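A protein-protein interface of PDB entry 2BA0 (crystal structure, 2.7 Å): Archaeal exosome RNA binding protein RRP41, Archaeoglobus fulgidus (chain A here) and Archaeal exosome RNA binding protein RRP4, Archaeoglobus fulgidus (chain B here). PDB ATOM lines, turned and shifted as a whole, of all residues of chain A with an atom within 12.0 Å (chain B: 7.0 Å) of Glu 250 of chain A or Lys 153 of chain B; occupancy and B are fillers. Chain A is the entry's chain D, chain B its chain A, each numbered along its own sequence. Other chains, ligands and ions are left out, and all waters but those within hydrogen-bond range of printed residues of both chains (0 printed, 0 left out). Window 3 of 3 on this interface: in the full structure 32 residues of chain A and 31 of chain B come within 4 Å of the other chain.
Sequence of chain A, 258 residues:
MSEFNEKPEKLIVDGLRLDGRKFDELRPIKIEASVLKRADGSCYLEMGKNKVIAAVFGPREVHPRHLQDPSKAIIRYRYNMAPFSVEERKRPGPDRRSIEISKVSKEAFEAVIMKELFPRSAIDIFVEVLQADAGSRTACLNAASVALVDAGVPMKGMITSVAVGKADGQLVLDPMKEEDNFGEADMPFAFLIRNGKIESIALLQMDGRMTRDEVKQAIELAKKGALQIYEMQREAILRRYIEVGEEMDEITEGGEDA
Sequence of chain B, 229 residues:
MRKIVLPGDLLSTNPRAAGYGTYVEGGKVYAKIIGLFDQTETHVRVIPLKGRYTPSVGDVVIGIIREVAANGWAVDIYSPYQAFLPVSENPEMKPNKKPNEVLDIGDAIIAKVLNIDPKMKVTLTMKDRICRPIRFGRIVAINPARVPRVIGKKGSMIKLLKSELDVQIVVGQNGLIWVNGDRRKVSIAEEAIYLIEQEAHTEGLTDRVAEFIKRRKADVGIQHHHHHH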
ATOM      1  N   TYR A 241     -18.888  -2.793  -8.771  1.00  0.00           N
ATOM      2  CA  TYR A 241     -20.215  -3.243  -9.172  1.00  0.00           C
ATOM      3  C   TYR A 241     -20.318  -4.296 -10.256  1.00  0.00           C
ATOM      4  O   TYR A 241     -21.423  -4.749 -10.561  1.00  0.00           O
ATOM      5  CB  TYR A 241     -21.076  -2.053  -9.592  1.00  0.00           C
ATOM      6  CG  TYR A 241     -21.714  -1.320  -8.438  1.00  0.00           C
ATOM      7  CD1 TYR A 241     -20.992  -0.394  -7.684  1.00  0.00           C
ATOM      8  CD2 TYR A 241     -23.030  -1.581  -8.072  1.00  0.00           C
ATOM      9  CE1 TYR A 241     -21.567   0.248  -6.590  1.00  0.00           C
ATOM     10  CE2 TYR A 241     -23.611  -0.951  -6.983  1.00  0.00           C
ATOM     11  CZ  TYR A 241     -22.876  -0.037  -6.246  1.00  0.00           C
ATOM     12  OH  TYR A 241     -23.450   0.584  -5.161  1.00  0.00           O
ATOM     13  N   ILE A 242     -19.197  -4.697 -10.842  1.00  0.00           N
ATOM     14  CA  ILE A 242     -19.248  -5.700 -11.902  1.00  0.00           C
ATOM     15  C   ILE A 242     -20.038  -6.945 -11.495  1.00  0.00           C
ATOM     16  O   ILE A 242     -20.862  -7.450 -12.260  1.00  0.00           O
ATOM     17  CB  ILE A 242     -17.842  -6.151 -12.331  1.00  0.00           C
ATOM     18  CG1 ILE A 242     -16.995  -4.936 -12.704  1.00  0.00           C
ATOM     19  CG2 ILE A 242     -17.943  -7.062 -13.537  1.00  0.00           C
ATOM     20  CD1 ILE A 242     -15.536  -5.267 -12.997  1.00  0.00           C
ATOM     21  N   GLU A 243     -19.792  -7.429 -10.285  1.00  0.00           N
ATOM     22  CA  GLU A 243     -20.454  -8.623  -9.796  1.00  0.00           C
ATOM     23  C   GLU A 243     -21.983  -8.522  -9.650  1.00  0.00           C
ATOM     24  O   GLU A 243     -22.701  -9.347 -10.215  1.00  0.00           O
ATOM     25  CB  GLU A 243     -19.806  -9.059  -8.480  1.00  0.00           C
ATOM     26  CG  GLU A 243     -20.339 -10.359  -7.939  1.00  0.00           C
ATOM     27  CD  GLU A 243     -19.501 -10.910  -6.804  1.00  0.00           C
ATOM     28  OE1 GLU A 243     -19.168 -10.137  -5.882  1.00  0.00           O
ATOM     29  OE2 GLU A 243     -19.184 -12.122  -6.834  1.00  0.00           O
ATOM     30  N   VAL A 244     -22.499  -7.538  -8.914  1.00  0.00           N
ATOM     31  CA  VAL A 244     -23.954  -7.435  -8.787  1.00  0.00           C
ATOM     32  C   VAL A 244     -24.601  -7.152 -10.131  1.00  0.00           C
ATOM     33  O   VAL A 244     -25.721  -7.586 -10.383  1.00  0.00           O
ATOM     34  CB  VAL A 244     -24.417  -6.320  -7.812  1.00  0.00           C
ATOM     35  CG1 VAL A 244     -24.238  -6.770  -6.386  1.00  0.00           C
ATOM     36  CG2 VAL A 244     -23.662  -5.038  -8.083  1.00  0.00           C
ATOM     37  N   GLY A 245     -23.907  -6.402 -10.980  1.00  0.00           N
ATOM     38  CA  GLY A 245     -24.444  -6.096 -12.293  1.00  0.00           C
ATOM     39  C   GLY A 245     -24.726  -7.385 -13.042  1.00  0.00           C
ATOM     40  O   GLY A 245     -25.796  -7.557 -13.642  1.00  0.00           O
ATOM     41  N   GLU A 246     -23.759  -8.299 -12.994  1.00  0.00           N
ATOM     42  CA  GLU A 246     -23.888  -9.584 -13.661  1.00  0.00           C
ATOM     43  C   GLU A 246     -25.024 -10.371 -13.050  1.00  0.00           C
ATOM     44  O   GLU A 246     -25.833 -10.977 -13.761  1.00  0.00           O
ATOM     45  CB  GLU A 246     -22.598 -10.387 -13.532  1.00  0.00           C
ATOM     46  CG  GLU A 246     -21.451  -9.839 -14.349  1.00  0.00           C
ATOM     47  CD  GLU A 246     -20.159 -10.614 -14.143  1.00  0.00           C
ATOM     48  OE1 GLU A 246     -19.122 -10.206 -14.717  1.00  0.00           O
ATOM     49  OE2 GLU A 246     -20.176 -11.629 -13.408  1.00  0.00           O
ATOM     50  N   GLU A 247     -25.078 -10.368 -11.724  1.00  0.00           N
ATOM     51  CA  GLU A 247     -26.127 -11.089 -11.040  1.00  0.00           C
ATOM     52  C   GLU A 247     -27.483 -10.571 -11.490  1.00  0.00           C
ATOM     53  O   GLU A 247     -28.374 -11.349 -11.813  1.00  0.00           O
ATOM     54  CB  GLU A 247     -26.004 -10.930  -9.528  1.00  0.00           C
ATOM     55  CG  GLU A 247     -27.086 -11.687  -8.774  1.00  0.00           C
ATOM     56  CD  GLU A 247     -27.181 -11.293  -7.318  1.00  0.00           C
ATOM     57  OE1 GLU A 247     -28.042 -11.865  -6.602  1.00  0.00           O
ATOM     58  OE2 GLU A 247     -26.397 -10.411  -6.894  1.00  0.00           O
ATOM     59  N   MET A 248     -27.642  -9.253 -11.508  1.00  0.00           N
ATOM     60  CA  MET A 248     -28.915  -8.675 -11.906  1.00  0.00           C
ATOM     61  C   MET A 248     -29.202  -9.061 -13.349  1.00  0.00           C
ATOM     62  O   MET A 248     -30.326  -9.439 -13.692  1.00  0.00           O
ATOM     63  CB  MET A 248     -28.878  -7.153 -11.768  1.00  0.00           C
ATOM     64  CG  MET A 248     -30.254  -6.496 -11.775  1.00  0.00           C
ATOM     65  SD  MET A 248     -31.231  -6.929 -10.312  1.00  0.00           S
ATOM     66  CE  MET A 248     -32.197  -8.274 -10.948  1.00  0.00           C
ATOM     67  N   ASP A 249     -28.176  -8.972 -14.192  1.00  0.00           N
ATOM     68  CA  ASP A 249     -28.328  -9.316 -15.601  1.00  0.00           C
ATOM     69  C   ASP A 249     -28.785 -10.765 -15.747  1.00  0.00           C
ATOM     70  O   ASP A 249     -29.646 -11.074 -16.565  1.00  0.00           O
ATOM     71  CB  ASP A 249     -27.010  -9.094 -16.355  1.00  0.00           C
ATOM     72  CG  ASP A 249     -27.217  -8.910 -17.846  1.00  0.00           C
ATOM     73  N   GLU A 250     -28.211 -11.655 -14.947  1.00  0.00           N
ATOM     74  CA  GLU A 250     -28.596 -13.057 -14.988  1.00  0.00           C
ATOM     75  C   GLU A 250     -30.064 -13.217 -14.566  1.00  0.00           C
ATOM     76  O   GLU A 250     -30.858 -13.821 -15.279  1.00  0.00           O
ATOM     77  CB  GLU A 250     -27.699 -13.867 -14.053  1.00  0.00           C
ATOM     78  CG  GLU A 250     -28.012 -15.350 -14.020  1.00  0.00           C
ATOM     79  CD  GLU A 250     -27.536 -16.079 -15.264  1.00  0.00           C
ATOM     80  OE1 GLU A 250     -28.356 -16.798 -15.884  1.00  0.00           O
ATOM     81  OE2 GLU A 250     -26.340 -15.936 -15.613  1.00  0.00           O
ATOM     82  N   ILE A 251     -30.415 -12.663 -13.407  1.00  0.00           N
ATOM     83  CA  ILE A 251     -31.776 -12.754 -12.872  1.00  0.00           C
ATOM     84  C   ILE A 251     -32.819 -12.131 -13.787  1.00  0.00           C
ATOM     85  O   ILE A 251     -33.881 -12.714 -14.015  1.00  0.00           O
ATOM     86  CB  ILE A 251     -31.897 -12.057 -11.488  1.00  0.00           C
ATOM     87  CG1 ILE A 251     -30.992 -12.745 -10.468  1.00  0.00           C
ATOM     88  CG2 ILE A 251     -33.337 -12.098 -11.007  1.00  0.00           C
ATOM     89  CD1 ILE A 251     -31.022 -12.115  -9.096  1.00  0.00           C
ATOM     90  N   THR A 252     -32.512 -10.942 -14.298  1.00  0.00           N
ATOM     91  CA  THR A 252     -33.422 -10.219 -15.173  1.00  0.00           C
ATOM     92  C   THR A 252     -33.320 -10.646 -16.626  1.00  0.00           C
ATOM     93  O   THR A 252     -34.380 -10.788 -17.268  1.00  0.00           O
ATOM     94  CB  THR A 252     -33.164  -8.714 -15.102  1.00  0.00           C
ATOM     95  OG1 THR A 252     -33.397  -8.252 -13.764  1.00  0.00           O
ATOM     96  CG2 THR A 252     -34.083  -7.973 -16.065  1.00  0.00           C
ATOM     97  N   ARG B   2     -24.959  -7.429 -21.083  1.00  0.00           N
ATOM     98  CA  ARG B   2     -25.630  -6.106 -20.827  1.00  0.00           C
ATOM     99  C   ARG B   2     -24.778  -5.173 -19.959  1.00  0.00           C
ATOM    100  O   ARG B   2     -24.533  -5.441 -18.787  1.00  0.00           O
ATOM    101  CB  ARG B   2     -26.993  -6.322 -20.174  1.00  0.00           C
ATOM    102  CG  ARG B   2     -27.915  -5.141 -20.309  1.00  0.00           C
ATOM    103  CD  ARG B   2     -29.331  -5.573 -20.652  1.00  0.00           C
ATOM    104  NE  ARG B   2     -29.893  -6.485 -19.667  1.00  0.00           N
ATOM    105  CZ  ARG B   2     -31.195  -6.676 -19.492  1.00  0.00           C
ATOM    106  NH1 ARG B   2     -31.634  -7.533 -18.578  1.00  0.00           N
ATOM    107  NH2 ARG B   2     -32.061  -5.992 -20.221  1.00  0.00           N
ATOM    108  N   LEU B  36     -27.970  -1.256 -14.993  1.00  0.00           N
ATOM    109  CA  LEU B  36     -27.802  -1.889 -16.305  1.00  0.00           C
ATOM    110  C   LEU B  36     -28.589  -1.126 -17.366  1.00  0.00           C
ATOM    111  O   LEU B  36     -29.751  -0.786 -17.160  1.00  0.00           O
ATOM    112  CB  LEU B  36     -28.307  -3.336 -16.283  1.00  0.00           C
ATOM    113  CG  LEU B  36     -27.549  -4.437 -15.539  1.00  0.00           C
ATOM    114  CD1 LEU B  36     -27.234  -4.004 -14.124  1.00  0.00           C
ATOM    115  CD2 LEU B  36     -28.407  -5.689 -15.511  1.00  0.00           C
ATOM    116  N   PRO B 148     -35.096  -8.872  -5.902  1.00  0.00           N
ATOM    117  CA  PRO B 148     -34.971  -9.689  -7.110  1.00  0.00           C
ATOM    118  C   PRO B 148     -34.114 -10.943  -6.916  1.00  0.00           C
ATOM    119  O   PRO B 148     -34.193 -11.881  -7.715  1.00  0.00           O
ATOM    120  CB  PRO B 148     -34.399  -8.706  -8.138  1.00  0.00           C
ATOM    121  CG  PRO B 148     -33.698  -7.673  -7.301  1.00  0.00           C
ATOM    122  CD  PRO B 148     -34.635  -7.493  -6.146  1.00  0.00           C
ATOM    123  N   ARG B 149     -33.314 -10.975  -5.852  1.00  0.00           N
ATOM    124  CA  ARG B 149     -32.477 -12.139  -5.584  1.00  0.00           C
ATOM    125  C   ARG B 149     -33.224 -13.281  -4.869  1.00  0.00           C
ATOM    126  O   ARG B 149     -32.945 -14.453  -5.125  1.00  0.00           O
ATOM    127  CB  ARG B 149     -31.246 -11.747  -4.759  1.00  0.00           C
ATOM    128  CG  ARG B 149     -30.368 -12.937  -4.398  1.00  0.00           C
ATOM    129  CD  ARG B 149     -29.325 -12.602  -3.357  1.00  0.00           C
ATOM    130  NE  ARG B 149     -28.304 -11.698  -3.869  1.00  0.00           N
ATOM    131  CZ  ARG B 149     -27.222 -11.324  -3.188  1.00  0.00           C
ATOM    132  NH1 ARG B 149     -26.346 -10.494  -3.742  1.00  0.00           N
ATOM    133  NH2 ARG B 149     -27.016 -11.781  -1.958  1.00  0.00           N
ATOM    134  N   ILE B 151     -36.310 -13.884  -5.221  1.00  0.00           N
ATOM    135  CA  ILE B 151     -37.268 -14.380  -6.193  1.00  0.00           C
ATOM    136  C   ILE B 151     -36.470 -15.157  -7.230  1.00  0.00           C
ATOM    137  O   ILE B 151     -36.876 -16.235  -7.648  1.00  0.00           O
ATOM    138  CB  ILE B 151     -38.047 -13.225  -6.858  1.00  0.00           C
ATOM    139  CG1 ILE B 151     -38.896 -12.521  -5.800  1.00  0.00           C
ATOM    140  CG2 ILE B 151     -38.945 -13.759  -7.977  1.00  0.00           C
ATOM    141  CD1 ILE B 151     -39.799 -11.453  -6.347  1.00  0.00           C
ATOM    142  N   GLY B 152     -35.323 -14.606  -7.620  1.00  0.00           N
ATOM    143  CA  GLY B 152     -34.458 -15.272  -8.585  1.00  0.00           C
ATOM    144  C   GLY B 152     -34.895 -15.313 -10.044  1.00  0.00           C
ATOM    145  O   GLY B 152     -35.934 -14.761 -10.421  1.00  0.00           O
ATOM    146  N   LYS B 153     -34.085 -15.979 -10.865  1.00  0.00           N
ATOM    147  CA  LYS B 153     -34.358 -16.112 -12.295  1.00  0.00           C
ATOM    148  C   LYS B 153     -35.637 -16.917 -12.549  1.00  0.00           C
ATOM    149  O   LYS B 153     -35.728 -18.101 -12.206  1.00  0.00           O
ATOM    150  CB  LYS B 153     -33.166 -16.775 -12.990  1.00  0.00           C
ATOM    151  CG  LYS B 153     -33.217 -16.740 -14.513  1.00  0.00           C
ATOM    152  CD  LYS B 153     -31.844 -17.083 -15.096  1.00  0.00           C
ATOM    153  CE  LYS B 153     -31.846 -17.154 -16.624  1.00  0.00           C
ATOM    154  NZ  LYS B 153     -30.512 -17.576 -17.168  1.00  0.00           N
ATOM    155  N   LYS B 154     -36.629 -16.259 -13.139  1.00  0.00           N
ATOM    156  CA  LYS B 154     -37.903 -16.900 -13.442  1.00  0.00           C
ATOM    157  C   LYS B 154     -38.609 -17.477 -12.205  1.00  0.00           C
ATOM    158  O   LYS B 154     -39.402 -18.420 -12.315  1.00  0.00           O
ATOM    159  CB  LYS B 154     -37.688 -18.000 -14.487  1.00  0.00           C
ATOM    160  CG  LYS B 154     -37.083 -17.493 -15.784  1.00  0.00           C
ATOM    161  CD  LYS B 154     -37.351 -18.445 -16.938  1.00  0.00           C
ATOM    162  CE  LYS B 154     -37.117 -17.758 -18.278  1.00  0.00           C
ATOM    163  NZ  LYS B 154     -37.657 -18.560 -19.417  1.00  0.00           N
ATOM    164  N   GLY B 155     -38.325 -16.903 -11.036  1.00  0.00           N
ATOM    165  CA  GLY B 155     -38.941 -17.366  -9.804  1.00  0.00           C
ATOM    166  C   GLY B 155     -38.313 -18.624  -9.221  1.00  0.00           C
ATOM    167  O   GLY B 155     -38.851 -19.218  -8.280  1.00  0.00           O
ATOM    168  N   SER B 156     -37.168 -19.027  -9.768  1.00  0.00           N
ATOM    169  CA  SER B 156     -36.479 -20.227  -9.306  1.00  0.00           C
ATOM    170  C   SER B 156     -36.169 -20.288  -7.802  1.00  0.00           C
ATOM    171  O   SER B 156     -36.165 -21.369  -7.217  1.00  0.00           O
ATOM    172  CB  SER B 156     -35.197 -20.435 -10.125  1.00  0.00           C
ATOM    173  OG  SER B 156     -34.500 -19.220 -10.335  1.00  0.00           O
ATOM    174  N   MET B 157     -35.916 -19.144  -7.171  1.00  0.00           N
ATOM    175  CA  MET B 157     -35.621 -19.121  -5.735  1.00  0.00           C
ATOM    176  C   MET B 157     -36.854 -19.321  -4.863  1.00  0.00           C
ATOM    177  O   MET B 157     -36.885 -20.231  -4.040  1.00  0.00           O
ATOM    178  CB  MET B 157     -34.944 -17.813  -5.336  1.00  0.00           C
ATOM    179  CG  MET B 157     -33.445 -17.918  -5.226  1.00  0.00           C
ATOM    180  SD  MET B 157     -32.903 -19.123  -3.985  1.00  0.00           S
ATOM    181  CE  MET B 157     -31.148 -19.022  -4.259  1.00  0.00           C
ATOM    182  N   LYS B 159     -39.544 -20.538  -5.634  1.00  0.00           N
ATOM    183  CA  LYS B 159     -40.053 -21.876  -5.908  1.00  0.00           C
ATOM    184  C   LYS B 159     -39.354 -22.887  -5.012  1.00  0.00           C
ATOM    185  O   LYS B 159     -40.010 -23.689  -4.347  1.00  0.00           O
ATOM    186  CB  LYS B 159     -39.849 -22.246  -7.378  1.00  0.00           C
ATOM    187  CG  LYS B 159     -40.793 -21.524  -8.340  1.00  0.00           C
ATOM    188  CD  LYS B 159     -40.438 -21.823  -9.791  1.00  0.00           C
ATOM    189  CE  LYS B 159     -41.188 -20.908 -10.743  1.00  0.00           C
ATOM    190  NZ  LYS B 159     -40.656 -21.006 -12.132  1.00  0.00           N
ATOM    191  N   THR B 206     -28.495 -21.021  -5.449  1.00  0.00           N
ATOM    192  CA  THR B 206     -29.696 -21.855  -5.515  1.00  0.00           C
ATOM    193  C   THR B 206     -29.431 -23.242  -4.939  1.00  0.00           C
ATOM    194  O   THR B 206     -30.297 -23.831  -4.291  1.00  0.00           O
ATOM    195  CB  THR B 206     -30.213 -22.028  -6.958  1.00  0.00           C
ATOM    196  OG1 THR B 206     -30.536 -20.749  -7.516  1.00  0.00           O
ATOM    197  CG2 THR B 206     -31.467 -22.894  -6.964  1.00  0.00           C
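OE1 of Glu 247 of chain A is in salt-bridge range of NE of Arg 149 of chain B (2.8 Å).
The side-chain amino group (NZ) of Lys 153 of chain B lies within salt-bridge range of the side-chain carboxylate (OE1) of Glu 250 of chain A (2.6 Å).
OG of Ser 156 of chain B sits at hydrogen-bond distance from O of Lys 153 of chain B, 2.5 Å away.
The backbone carbonyl oxygen (O) of Met 248 of chain A lies close to the side-chain hydroxyl (OG1) of Thr 252 of chain A, 3.3 Å away.
Gly 245 of chain A touches Leu 36 of chain B (O to CD2, 3.7 Å).
Met 248 of chain A touches Pro 148 of chain B.
Arg 2 of chain B touches Asp 249 of chain A (CB to CG, 3.5 Å).
CD2 of Leu 36 of chain B touches N of Asp 249 of chain A, at 3.5 Å.
Pro 148 of chain B touches Ile 251 of chain A.
CD1 of Ile 251 of chain A touches CA of Arg 149 of chain B, at 3.8 Å.
Gly 152 of chain B touches Ile 251 of chain A.
Ile 251 of chain A touches Lys 153 of chain B (O to CA, 3.8 Å).
NH1 of Arg 2 of chain B touches CG2 of Thr 252 of chain A, 3.5 Å away.
Lys 153 of chain B touches just these residues of chain A: Glu 250 and Ile 251.
Gly 152 of chain B touches one residue of chain A.
No residue of chain A comes within 4 Å of Gly 155 of chain B.
No residue of chain A comes within 4 Å of Ser 156 of chain B.
Printed residues of chain B within 4 Å of Thr 252 of chain A: Arg 2.
Printed residues of chain A within 4 Å of Leu 36 of chain B: Gly 245 (3.7 Å) and Asp 249 (3.5 Å).
Printed residues of chain A within 4 Å of Pro 148 of chain B: Met 248 (3.6 Å) and Ile 251 (3.4 Å).
Lys 159 of chain B touches none of the printed residues of chain A.
The nearest residue of chain B that does not touch Glu 250 of chain A is Leu 36 of chain B (6.0 Å).
The nearest printed residue of chain A that does not touch Leu 36 of chain B is Met 248 of chain A (4.05 Å).
Of the 12 printed residues of chain A, 7 touch a printed residue of chain B.
Hydrophobic or aromatic side chains of chain A that line the printed part of chain B: Met 248 and Ile 251.
Of the 13 printed residues of chain B, 6 touch a printed residue of chain A.
Printed residues of chain B that touch a printed residue of chain A: Arg 2, Leu 36, Pro 148, Arg 149, Gly 152 and Lys 153.
Among the printed residues, Asp or Glu carboxylates within 4 Å of a Lys or Arg side-chain nitrogen of the other chain: Glu 247 of chain A with Arg 149 of chain B (2.8 Å) and Glu 250 of chain A with Lys 153 of chain B (2.6 Å).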
